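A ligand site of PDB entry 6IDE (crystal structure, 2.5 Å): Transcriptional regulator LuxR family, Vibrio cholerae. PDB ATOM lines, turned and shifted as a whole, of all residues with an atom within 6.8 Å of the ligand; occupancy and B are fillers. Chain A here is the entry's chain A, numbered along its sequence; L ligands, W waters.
The side-chain amino group of Lys 24 sits at hydrogen-bond distance from an oxygen (O1) of the ligand (3.3 Å).
OH of Tyr 37 sits at hydrogen-bond distance from N2 of the ligand, 2.8 Å away.
NZ of Lys 102 sits at hydrogen-bond distance from O1 of the ligand, 2.5 Å away.
OD1 of Asp 86 lies within hydrogen-bond range of NE2 of His 88, at 2.7 Å.
NZ of Lys 102 lies within salt-bridge range of OD1 of Asp 72, at 3.2 Å.
The side-chain hydroxyl (OG) of Ser 230 lies within hydrogen-bond range of the side-chain carboxylate (OD1) of Asp 86.
NZ of Lys 102 lies within hydrogen-bond range of O of Phe 68.
NZ of Lys 24 is in salt-bridge range of OD2 of Asp 72, 2.7 Å away.
NZ of Lys 102 is in hydrogen-bond range of OE1 of Gln 71 (3.1 Å).
N of His 98 sits at hydrogen-bond distance from O of Asp 86, at 2.8 Å.
The side-chain amino group of Lys 24 is in salt-bridge range of the side-chain carboxylate of Asp 54 (2.9 Å).
Residues that only touch the ligand: Phe 68 (3.2 Å), Asp 54 (3.3 Å), Tyr 90 (3.3 Å), Asp 86 (3.5 Å), Phe 30 (3.6 Å) and Phe 100 (3.6 Å).
Hydrophobic or aromatic side chains that line the ligand: Phe 30, Tyr 37, Phe 68 and Phe 100.
Nine residues have an atom within 4 Å of the ligand: Lys 24, Phe 30, Tyr 37, Asp 54, Phe 68, Asp 86, Tyr 90, Phe 100 and Lys 102.
Along chain A the residues within 4 Å of the ligand span positions 24 to 102.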
ATOM      1  N   LYS A  24       4.524   4.678 -28.012  1.00  0.00           N
ATOM      2  CA  LYS A  24       5.045   5.800 -28.764  1.00  0.00           C
ATOM      3  C   LYS A  24       6.571   5.712 -28.765  1.00  0.00           C
ATOM      4  O   LYS A  24       7.159   5.145 -27.840  1.00  0.00           O
ATOM      5  CB  LYS A  24       4.572   7.142 -28.170  1.00  0.00           C
ATOM      6  CG  LYS A  24       3.066   7.311 -28.210  1.00  0.00           C
ATOM      7  CD  LYS A  24       2.604   8.619 -27.627  1.00  0.00           C
ATOM      8  CE  LYS A  24       2.641   8.597 -26.121  1.00  0.00           C
ATOM      9  NZ  LYS A  24       1.997   9.806 -25.534  1.00  0.00           N
ATOM     10  N   PHE A  30       3.042   8.111 -32.253  1.00  0.00           N
ATOM     11  CA  PHE A  30       2.330   6.869 -31.996  1.00  0.00           C
ATOM     12  C   PHE A  30       2.833   5.760 -32.916  1.00  0.00           C
ATOM     13  O   PHE A  30       2.802   5.896 -34.136  1.00  0.00           O
ATOM     14  CB  PHE A  30       0.828   7.071 -32.184  1.00  0.00           C
ATOM     15  CG  PHE A  30       0.122   7.611 -30.984  1.00  0.00           C
ATOM     16  CD1 PHE A  30       0.257   8.939 -30.621  1.00  0.00           C
ATOM     17  CD2 PHE A  30      -0.692   6.793 -30.218  1.00  0.00           C
ATOM     18  CE1 PHE A  30      -0.388   9.434 -29.516  1.00  0.00           C
ATOM     19  CE2 PHE A  30      -1.353   7.287 -29.107  1.00  0.00           C
ATOM     20  CZ  PHE A  30      -1.199   8.611 -28.758  1.00  0.00           C
ATOM     21  N   TYR A  37      -8.513   2.673 -27.657  1.00  0.00           N
ATOM     22  CA  TYR A  37      -7.953   4.015 -27.589  1.00  0.00           C
ATOM     23  C   TYR A  37      -8.278   4.824 -28.826  1.00  0.00           C
ATOM     24  O   TYR A  37      -8.657   5.990 -28.724  1.00  0.00           O
ATOM     25  CB  TYR A  37      -6.438   3.943 -27.389  1.00  0.00           C
ATOM     26  CG  TYR A  37      -5.837   5.317 -27.221  1.00  0.00           C
ATOM     27  CD1 TYR A  37      -5.835   5.932 -25.970  1.00  0.00           C
ATOM     28  CD2 TYR A  37      -5.308   6.008 -28.293  1.00  0.00           C
ATOM     29  CE1 TYR A  37      -5.306   7.198 -25.805  1.00  0.00           C
ATOM     30  CE2 TYR A  37      -4.771   7.278 -28.139  1.00  0.00           C
ATOM     31  CZ  TYR A  37      -4.766   7.869 -26.884  1.00  0.00           C
ATOM     32  OH  TYR A  37      -4.233   9.131 -26.727  1.00  0.00           O
ATOM     33  N   LEU A  40     -11.764   6.109 -28.406  1.00  0.00           N
ATOM     34  CA  LEU A  40     -11.798   7.131 -27.366  1.00  0.00           C
ATOM     35  C   LEU A  40     -11.324   8.487 -27.894  1.00  0.00           C
ATOM     36  O   LEU A  40     -11.857   9.530 -27.493  1.00  0.00           O
ATOM     37  CB  LEU A  40     -10.927   6.680 -26.193  1.00  0.00           C
ATOM     38  CG  LEU A  40     -10.628   7.734 -25.135  1.00  0.00           C
ATOM     39  CD1 LEU A  40     -11.878   8.038 -24.330  1.00  0.00           C
ATOM     40  CD2 LEU A  40      -9.487   7.252 -24.238  1.00  0.00           C
ATOM     41  N   ILE A  41     -10.347   8.479 -28.798  1.00  0.00           N
ATOM     42  CA  ILE A  41      -9.750   9.703 -29.325  1.00  0.00           C
ATOM     43  C   ILE A  41     -10.486  10.247 -30.545  1.00  0.00           C
ATOM     44  O   ILE A  41     -10.379  11.433 -30.855  1.00  0.00           O
ATOM     45  CB  ILE A  41      -8.261   9.445 -29.642  1.00  0.00           C
ATOM     46  CG1 ILE A  41      -7.457   9.419 -28.351  1.00  0.00           C
ATOM     47  CG2 ILE A  41      -7.681  10.467 -30.570  1.00  0.00           C
ATOM     48  CD1 ILE A  41      -7.546  10.706 -27.544  1.00  0.00           C
ATOM     49  N   ASP A  54       0.425  13.527 -30.023  1.00  0.00           N
ATOM     50  CA  ASP A  54      -0.738  13.894 -29.218  1.00  0.00           C
ATOM     51  C   ASP A  54      -1.345  15.212 -29.661  1.00  0.00           C
ATOM     52  O   ASP A  54      -2.516  15.468 -29.374  1.00  0.00           O
ATOM     53  CB  ASP A  54      -0.332  13.954 -27.733  1.00  0.00           C
ATOM     54  CG  ASP A  54      -0.040  12.569 -27.137  1.00  0.00           C
ATOM     55  OD1 ASP A  54      -0.957  11.732 -27.068  1.00  0.00           O
ATOM     56  OD2 ASP A  54       1.126  12.315 -26.754  1.00  0.00           O
ATOM     57  N   SER A  59      -9.316  15.359 -30.975  1.00  0.00           N
ATOM     58  CA  SER A  59      -9.861  15.235 -29.635  1.00  0.00           C
ATOM     59  C   SER A  59      -9.499  16.490 -28.853  1.00  0.00           C
ATOM     60  O   SER A  59      -8.427  17.073 -29.097  1.00  0.00           O
ATOM     61  CB  SER A  59      -9.316  13.983 -28.930  1.00  0.00           C
ATOM     62  OG  SER A  59      -9.344  14.111 -27.511  1.00  0.00           O
ATOM     63  N   THR A  61      -8.426  16.464 -26.012  1.00  0.00           N
ATOM     64  CA  THR A  61      -7.223  16.104 -25.265  1.00  0.00           C
ATOM     65  C   THR A  61      -5.962  16.681 -25.876  1.00  0.00           C
ATOM     66  O   THR A  61      -4.934  16.754 -25.179  1.00  0.00           O
ATOM     67  CB  THR A  61      -7.073  14.584 -25.171  1.00  0.00           C
ATOM     68  OG1 THR A  61      -7.174  14.006 -26.479  1.00  0.00           O
ATOM     69  CG2 THR A  61      -8.142  13.993 -24.273  1.00  0.00           C
ATOM     70  N   CYS A  64      -3.745  19.229 -24.014  1.00  0.00           N
ATOM     71  CA  CYS A  64      -2.805  18.820 -22.976  1.00  0.00           C
ATOM     72  C   CYS A  64      -1.639  18.006 -23.534  1.00  0.00           C
ATOM     73  O   CYS A  64      -0.925  17.359 -22.768  1.00  0.00           O
ATOM     74  CB  CYS A  64      -3.528  18.018 -21.885  1.00  0.00           C
ATOM     75  SG  CYS A  64      -4.711  18.992 -20.927  1.00  0.00           S
ATOM     76  N   GLU A  67       1.706  18.252 -21.761  1.00  0.00           N
ATOM     77  CA  GLU A  67       1.850  17.513 -20.514  1.00  0.00           C
ATOM     78  C   GLU A  67       2.145  16.044 -20.792  1.00  0.00           C
ATOM     79  O   GLU A  67       3.038  15.462 -20.174  1.00  0.00           O
ATOM     80  CB  GLU A  67       0.593  17.655 -19.646  1.00  0.00           C
ATOM     81  CG  GLU A  67       0.446  19.035 -19.001  1.00  0.00           C
ATOM     82  CD  GLU A  67      -0.353  20.010 -19.850  1.00  0.00           C
ATOM     83  OE1 GLU A  67      -1.530  20.278 -19.510  1.00  0.00           O
ATOM     84  OE2 GLU A  67       0.210  20.508 -20.860  1.00  0.00           O
ATOM     85  N   PHE A  68       1.424  15.460 -21.759  1.00  0.00           N
ATOM     86  CA  PHE A  68       1.666  14.081 -22.170  1.00  0.00           C
ATOM     87  C   PHE A  68       3.129  13.872 -22.543  1.00  0.00           C
ATOM     88  O   PHE A  68       3.776  12.932 -22.054  1.00  0.00           O
ATOM     89  CB  PHE A  68       0.763  13.724 -23.354  1.00  0.00           C
ATOM     90  CG  PHE A  68      -0.715  13.863 -23.082  1.00  0.00           C
ATOM     91  CD1 PHE A  68      -1.205  14.024 -21.796  1.00  0.00           C
ATOM     92  CD2 PHE A  68      -1.630  13.805 -24.130  1.00  0.00           C
ATOM     93  CE1 PHE A  68      -2.570  14.127 -21.564  1.00  0.00           C
ATOM     94  CE2 PHE A  68      -2.987  13.925 -23.906  1.00  0.00           C
ATOM     95  CZ  PHE A  68      -3.461  14.087 -22.625  1.00  0.00           C
ATOM     96  N   GLN A  69       3.672  14.729 -23.396  1.00  0.00           N
ATOM     97  CA  GLN A  69       5.046  14.523 -23.838  1.00  0.00           C
ATOM     98  C   GLN A  69       6.035  14.759 -22.704  1.00  0.00           C
ATOM     99  O   GLN A  69       7.060  14.077 -22.610  1.00  0.00           O
ATOM    100  CB  GLN A  69       5.350  15.420 -25.030  1.00  0.00           C
ATOM    101  CG  GLN A  69       4.403  15.231 -26.175  1.00  0.00           C
ATOM    102  CD  GLN A  69       4.789  16.024 -27.403  1.00  0.00           C
ATOM    103  OE1 GLN A  69       5.283  17.160 -27.311  1.00  0.00           O
ATOM    104  NE2 GLN A  69       4.559  15.440 -28.563  1.00  0.00           N
ATOM    105  N   GLN A  71       5.445  14.029 -19.524  1.00  0.00           N
ATOM    106  CA  GLN A  71       5.419  12.760 -18.794  1.00  0.00           C
ATOM    107  C   GLN A  71       6.160  11.676 -19.568  1.00  0.00           C
ATOM    108  O   GLN A  71       6.897  10.877 -18.974  1.00  0.00           O
ATOM    109  CB  GLN A  71       3.972  12.339 -18.521  1.00  0.00           C
ATOM    110  CG  GLN A  71       3.162  13.380 -17.790  1.00  0.00           C
ATOM    111  CD  GLN A  71       1.695  13.308 -18.143  1.00  0.00           C
ATOM    112  OE1 GLN A  71       1.285  12.486 -18.968  1.00  0.00           O
ATOM    113  NE2 GLN A  71       0.892  14.161 -17.517  1.00  0.00           N
ATOM    114  N   ASP A  72       5.978  11.652 -20.896  1.00  0.00           N
ATOM    115  CA  ASP A  72       6.709  10.682 -21.723  1.00  0.00           C
ATOM    116  C   ASP A  72       8.220  10.840 -21.544  1.00  0.00           C
ATOM    117  O   ASP A  72       8.926   9.862 -21.283  1.00  0.00           O
ATOM    118  CB  ASP A  72       6.329  10.850 -23.200  1.00  0.00           C
ATOM    119  CG  ASP A  72       4.926  10.327 -23.504  1.00  0.00           C
ATOM    120  OD1 ASP A  72       4.359   9.532 -22.702  1.00  0.00           O
ATOM    121  OD2 ASP A  72       4.385  10.716 -24.574  1.00  0.00           O
ATOM    122  N   VAL A  84      -0.495   8.665 -14.006  1.00  0.00           N
ATOM    123  CA  VAL A  84      -1.050   9.959 -14.385  1.00  0.00           C
ATOM    124  C   VAL A  84      -2.565   9.919 -14.221  1.00  0.00           C
ATOM    125  O   VAL A  84      -3.223   9.037 -14.766  1.00  0.00           O
ATOM    126  CB  VAL A  84      -0.700  10.336 -15.836  1.00  0.00           C
ATOM    127  CG1 VAL A  84      -1.269  11.710 -16.183  1.00  0.00           C
ATOM    128  CG2 VAL A  84       0.806  10.285 -16.061  1.00  0.00           C
ATOM    129  N   ASP A  86      -5.934  11.657 -15.408  1.00  0.00           N
ATOM    130  CA  ASP A  86      -6.358  12.352 -16.606  1.00  0.00           C
ATOM    131  C   ASP A  86      -7.853  12.641 -16.540  1.00  0.00           C
ATOM    132  O   ASP A  86      -8.649  11.733 -16.267  1.00  0.00           O
ATOM    133  CB  ASP A  86      -6.026  11.537 -17.855  1.00  0.00           C
ATOM    134  CG  ASP A  86      -4.643  11.848 -18.418  1.00  0.00           C
ATOM    135  OD1 ASP A  86      -4.390  13.031 -18.734  1.00  0.00           O
ATOM    136  OD2 ASP A  86      -3.800  10.936 -18.529  1.00  0.00           O
ATOM    137  N   HIS A  88     -10.624  14.820 -18.951  1.00  0.00           N
ATOM    138  CA  HIS A  88     -10.716  15.525 -20.217  1.00  0.00           C
ATOM    139  C   HIS A  88     -12.094  15.312 -20.809  1.00  0.00           C
ATOM    140  O   HIS A  88     -12.761  14.314 -20.509  1.00  0.00           O
ATOM    141  CB  HIS A  88      -9.649  15.041 -21.223  1.00  0.00           C
ATOM    142  CG  HIS A  88      -8.251  15.015 -20.699  1.00  0.00           C
ATOM    143  ND1 HIS A  88      -7.405  16.100 -20.769  1.00  0.00           N
ATOM    144  CD2 HIS A  88      -7.544  14.026 -20.113  1.00  0.00           C
ATOM    145  CE1 HIS A  88      -6.239  15.776 -20.239  1.00  0.00           C
ATOM    146  NE2 HIS A  88      -6.299  14.521 -19.838  1.00  0.00           N
ATOM    147  N   TYR A  90     -13.968  14.327 -24.421  1.00  0.00           N
ATOM    148  CA  TYR A  90     -13.598  13.485 -25.546  1.00  0.00           C
ATOM    149  C   TYR A  90     -14.614  13.626 -26.665  1.00  0.00           C
ATOM    150  O   TYR A  90     -15.716  14.126 -26.450  1.00  0.00           O
ATOM    151  CB  TYR A  90     -13.498  12.015 -25.100  1.00  0.00           C
ATOM    152  CG  TYR A  90     -12.273  11.765 -24.286  1.00  0.00           C
ATOM    153  CD1 TYR A  90     -12.239  12.052 -22.926  1.00  0.00           C
ATOM    154  CD2 TYR A  90     -11.129  11.268 -24.878  1.00  0.00           C
ATOM    155  CE1 TYR A  90     -11.085  11.835 -22.178  1.00  0.00           C
ATOM    156  CE2 TYR A  90      -9.989  11.031 -24.136  1.00  0.00           C
ATOM    157  CZ  TYR A  90      -9.975  11.319 -22.799  1.00  0.00           C
ATOM    158  OH  TYR A  90      -8.823  11.099 -22.089  1.00  0.00           O
ATOM    159  N   HIS A  98      -9.522   9.120 -16.423  1.00  0.00           N
ATOM    160  CA  HIS A  98      -8.692   7.939 -16.599  1.00  0.00           C
ATOM    161  C   HIS A  98      -7.469   8.016 -15.713  1.00  0.00           C
ATOM    162  O   HIS A  98      -7.020   9.097 -15.315  1.00  0.00           O
ATOM    163  CB  HIS A  98      -8.229   7.783 -18.054  1.00  0.00           C
ATOM    164  CG  HIS A  98      -9.352   7.643 -19.031  1.00  0.00           C
ATOM    165  ND1 HIS A  98      -9.605   6.473 -19.702  1.00  0.00           N
ATOM    166  CD2 HIS A  98     -10.279   8.534 -19.453  1.00  0.00           C
ATOM    167  CE1 HIS A  98     -10.656   6.644 -20.500  1.00  0.00           C
ATOM    168  NE2 HIS A  98     -11.073   7.889 -20.365  1.00  0.00           N
ATOM    169  N   PHE A 100      -3.795   6.835 -16.494  1.00  0.00           N
ATOM    170  CA  PHE A 100      -2.847   6.306 -17.461  1.00  0.00           C
ATOM    171  C   PHE A 100      -1.544   5.935 -16.763  1.00  0.00           C
ATOM    172  O   PHE A 100      -0.959   6.743 -16.052  1.00  0.00           O
ATOM    173  CB  PHE A 100      -2.598   7.293 -18.584  1.00  0.00           C
ATOM    174  CG  PHE A 100      -3.667   7.314 -19.626  1.00  0.00           C
ATOM    175  CD1 PHE A 100      -4.768   8.142 -19.479  1.00  0.00           C
ATOM    176  CD2 PHE A 100      -3.557   6.546 -20.766  1.00  0.00           C
ATOM    177  CE1 PHE A 100      -5.756   8.174 -20.452  1.00  0.00           C
ATOM    178  CE2 PHE A 100      -4.544   6.591 -21.735  1.00  0.00           C
ATOM    179  CZ  PHE A 100      -5.637   7.399 -21.571  1.00  0.00           C
ATOM    180  N   LYS A 102       2.290   4.756 -17.433  1.00  0.00           N
ATOM    181  CA  LYS A 102       3.276   4.909 -18.485  1.00  0.00           C
ATOM    182  C   LYS A 102       4.579   4.275 -18.027  1.00  0.00           C
ATOM    183  O   LYS A 102       5.012   4.501 -16.889  1.00  0.00           O
ATOM    184  CB  LYS A 102       3.487   6.392 -18.847  1.00  0.00           C
ATOM    185  CG  LYS A 102       2.239   7.069 -19.396  1.00  0.00           C
ATOM    186  CD  LYS A 102       2.493   8.528 -19.761  1.00  0.00           C
ATOM    187  CE  LYS A 102       1.261   9.116 -20.450  1.00  0.00           C
ATOM    188  NZ  LYS A 102       1.600  10.380 -21.223  1.00  0.00           N
ATOM    189  N   PHE A 117       1.851   3.403 -22.894  1.00  0.00           N
ATOM    190  CA  PHE A 117       0.787   3.945 -22.064  1.00  0.00           C
ATOM    191  C   PHE A 117      -0.307   2.889 -21.874  1.00  0.00           C
ATOM    192  O   PHE A 117      -0.543   2.031 -22.722  1.00  0.00           O
ATOM    193  CB  PHE A 117       0.214   5.227 -22.673  1.00  0.00           C
ATOM    194  CG  PHE A 117      -0.418   5.053 -24.012  1.00  0.00           C
ATOM    195  CD1 PHE A 117       0.349   5.078 -25.149  1.00  0.00           C
ATOM    196  CD2 PHE A 117      -1.784   4.907 -24.131  1.00  0.00           C
ATOM    197  CE1 PHE A 117      -0.233   4.940 -26.399  1.00  0.00           C
ATOM    198  CE2 PHE A 117      -2.374   4.770 -25.386  1.00  0.00           C
ATOM    199  CZ  PHE A 117      -1.595   4.770 -26.514  1.00  0.00           C
ATOM    200  N   SER A 230      -4.081  16.763 -16.307  1.00  0.00           N
ATOM    201  CA  SER A 230      -3.169  15.657 -16.607  1.00  0.00           C
ATOM    202  C   SER A 230      -1.969  15.828 -15.664  1.00  0.00           C
ATOM    203  O   SER A 230      -1.001  16.524 -15.989  1.00  0.00           O
ATOM    204  CB  SER A 230      -2.751  15.653 -18.064  1.00  0.00           C
ATOM    205  OG  SER A 230      -1.875  14.562 -18.339  1.00  0.00           O
HETATM  206  C1  LIG L   1      -3.533  10.917 -22.044  1.00  0.00           C
HETATM  207  C2  LIG L   1      -4.236  10.426 -23.139  1.00  0.00           C
HETATM  208  C3  LIG L   1      -2.291   9.729 -24.097  1.00  0.00           C
HETATM  209  C4  LIG L   1      -1.592  10.230 -23.011  1.00  0.00           C
HETATM  210  C5  LIG L   1      -5.753  10.562 -23.214  1.00  0.00           C
HETATM  211  C6  LIG L   1      -1.554   9.052 -25.247  1.00  0.00           C
HETATM  212  N1  LIG L   1      -2.214  10.816 -22.005  1.00  0.00           N
HETATM  213  N2  LIG L   1      -3.602   9.847 -24.143  1.00  0.00           N
HETATM  214  O1  LIG L   1      -0.185  10.093 -23.011  1.00  0.00           O
HETATM  215  O   HOH W   1      -1.012  11.074 -19.476  1.00  0.00           O
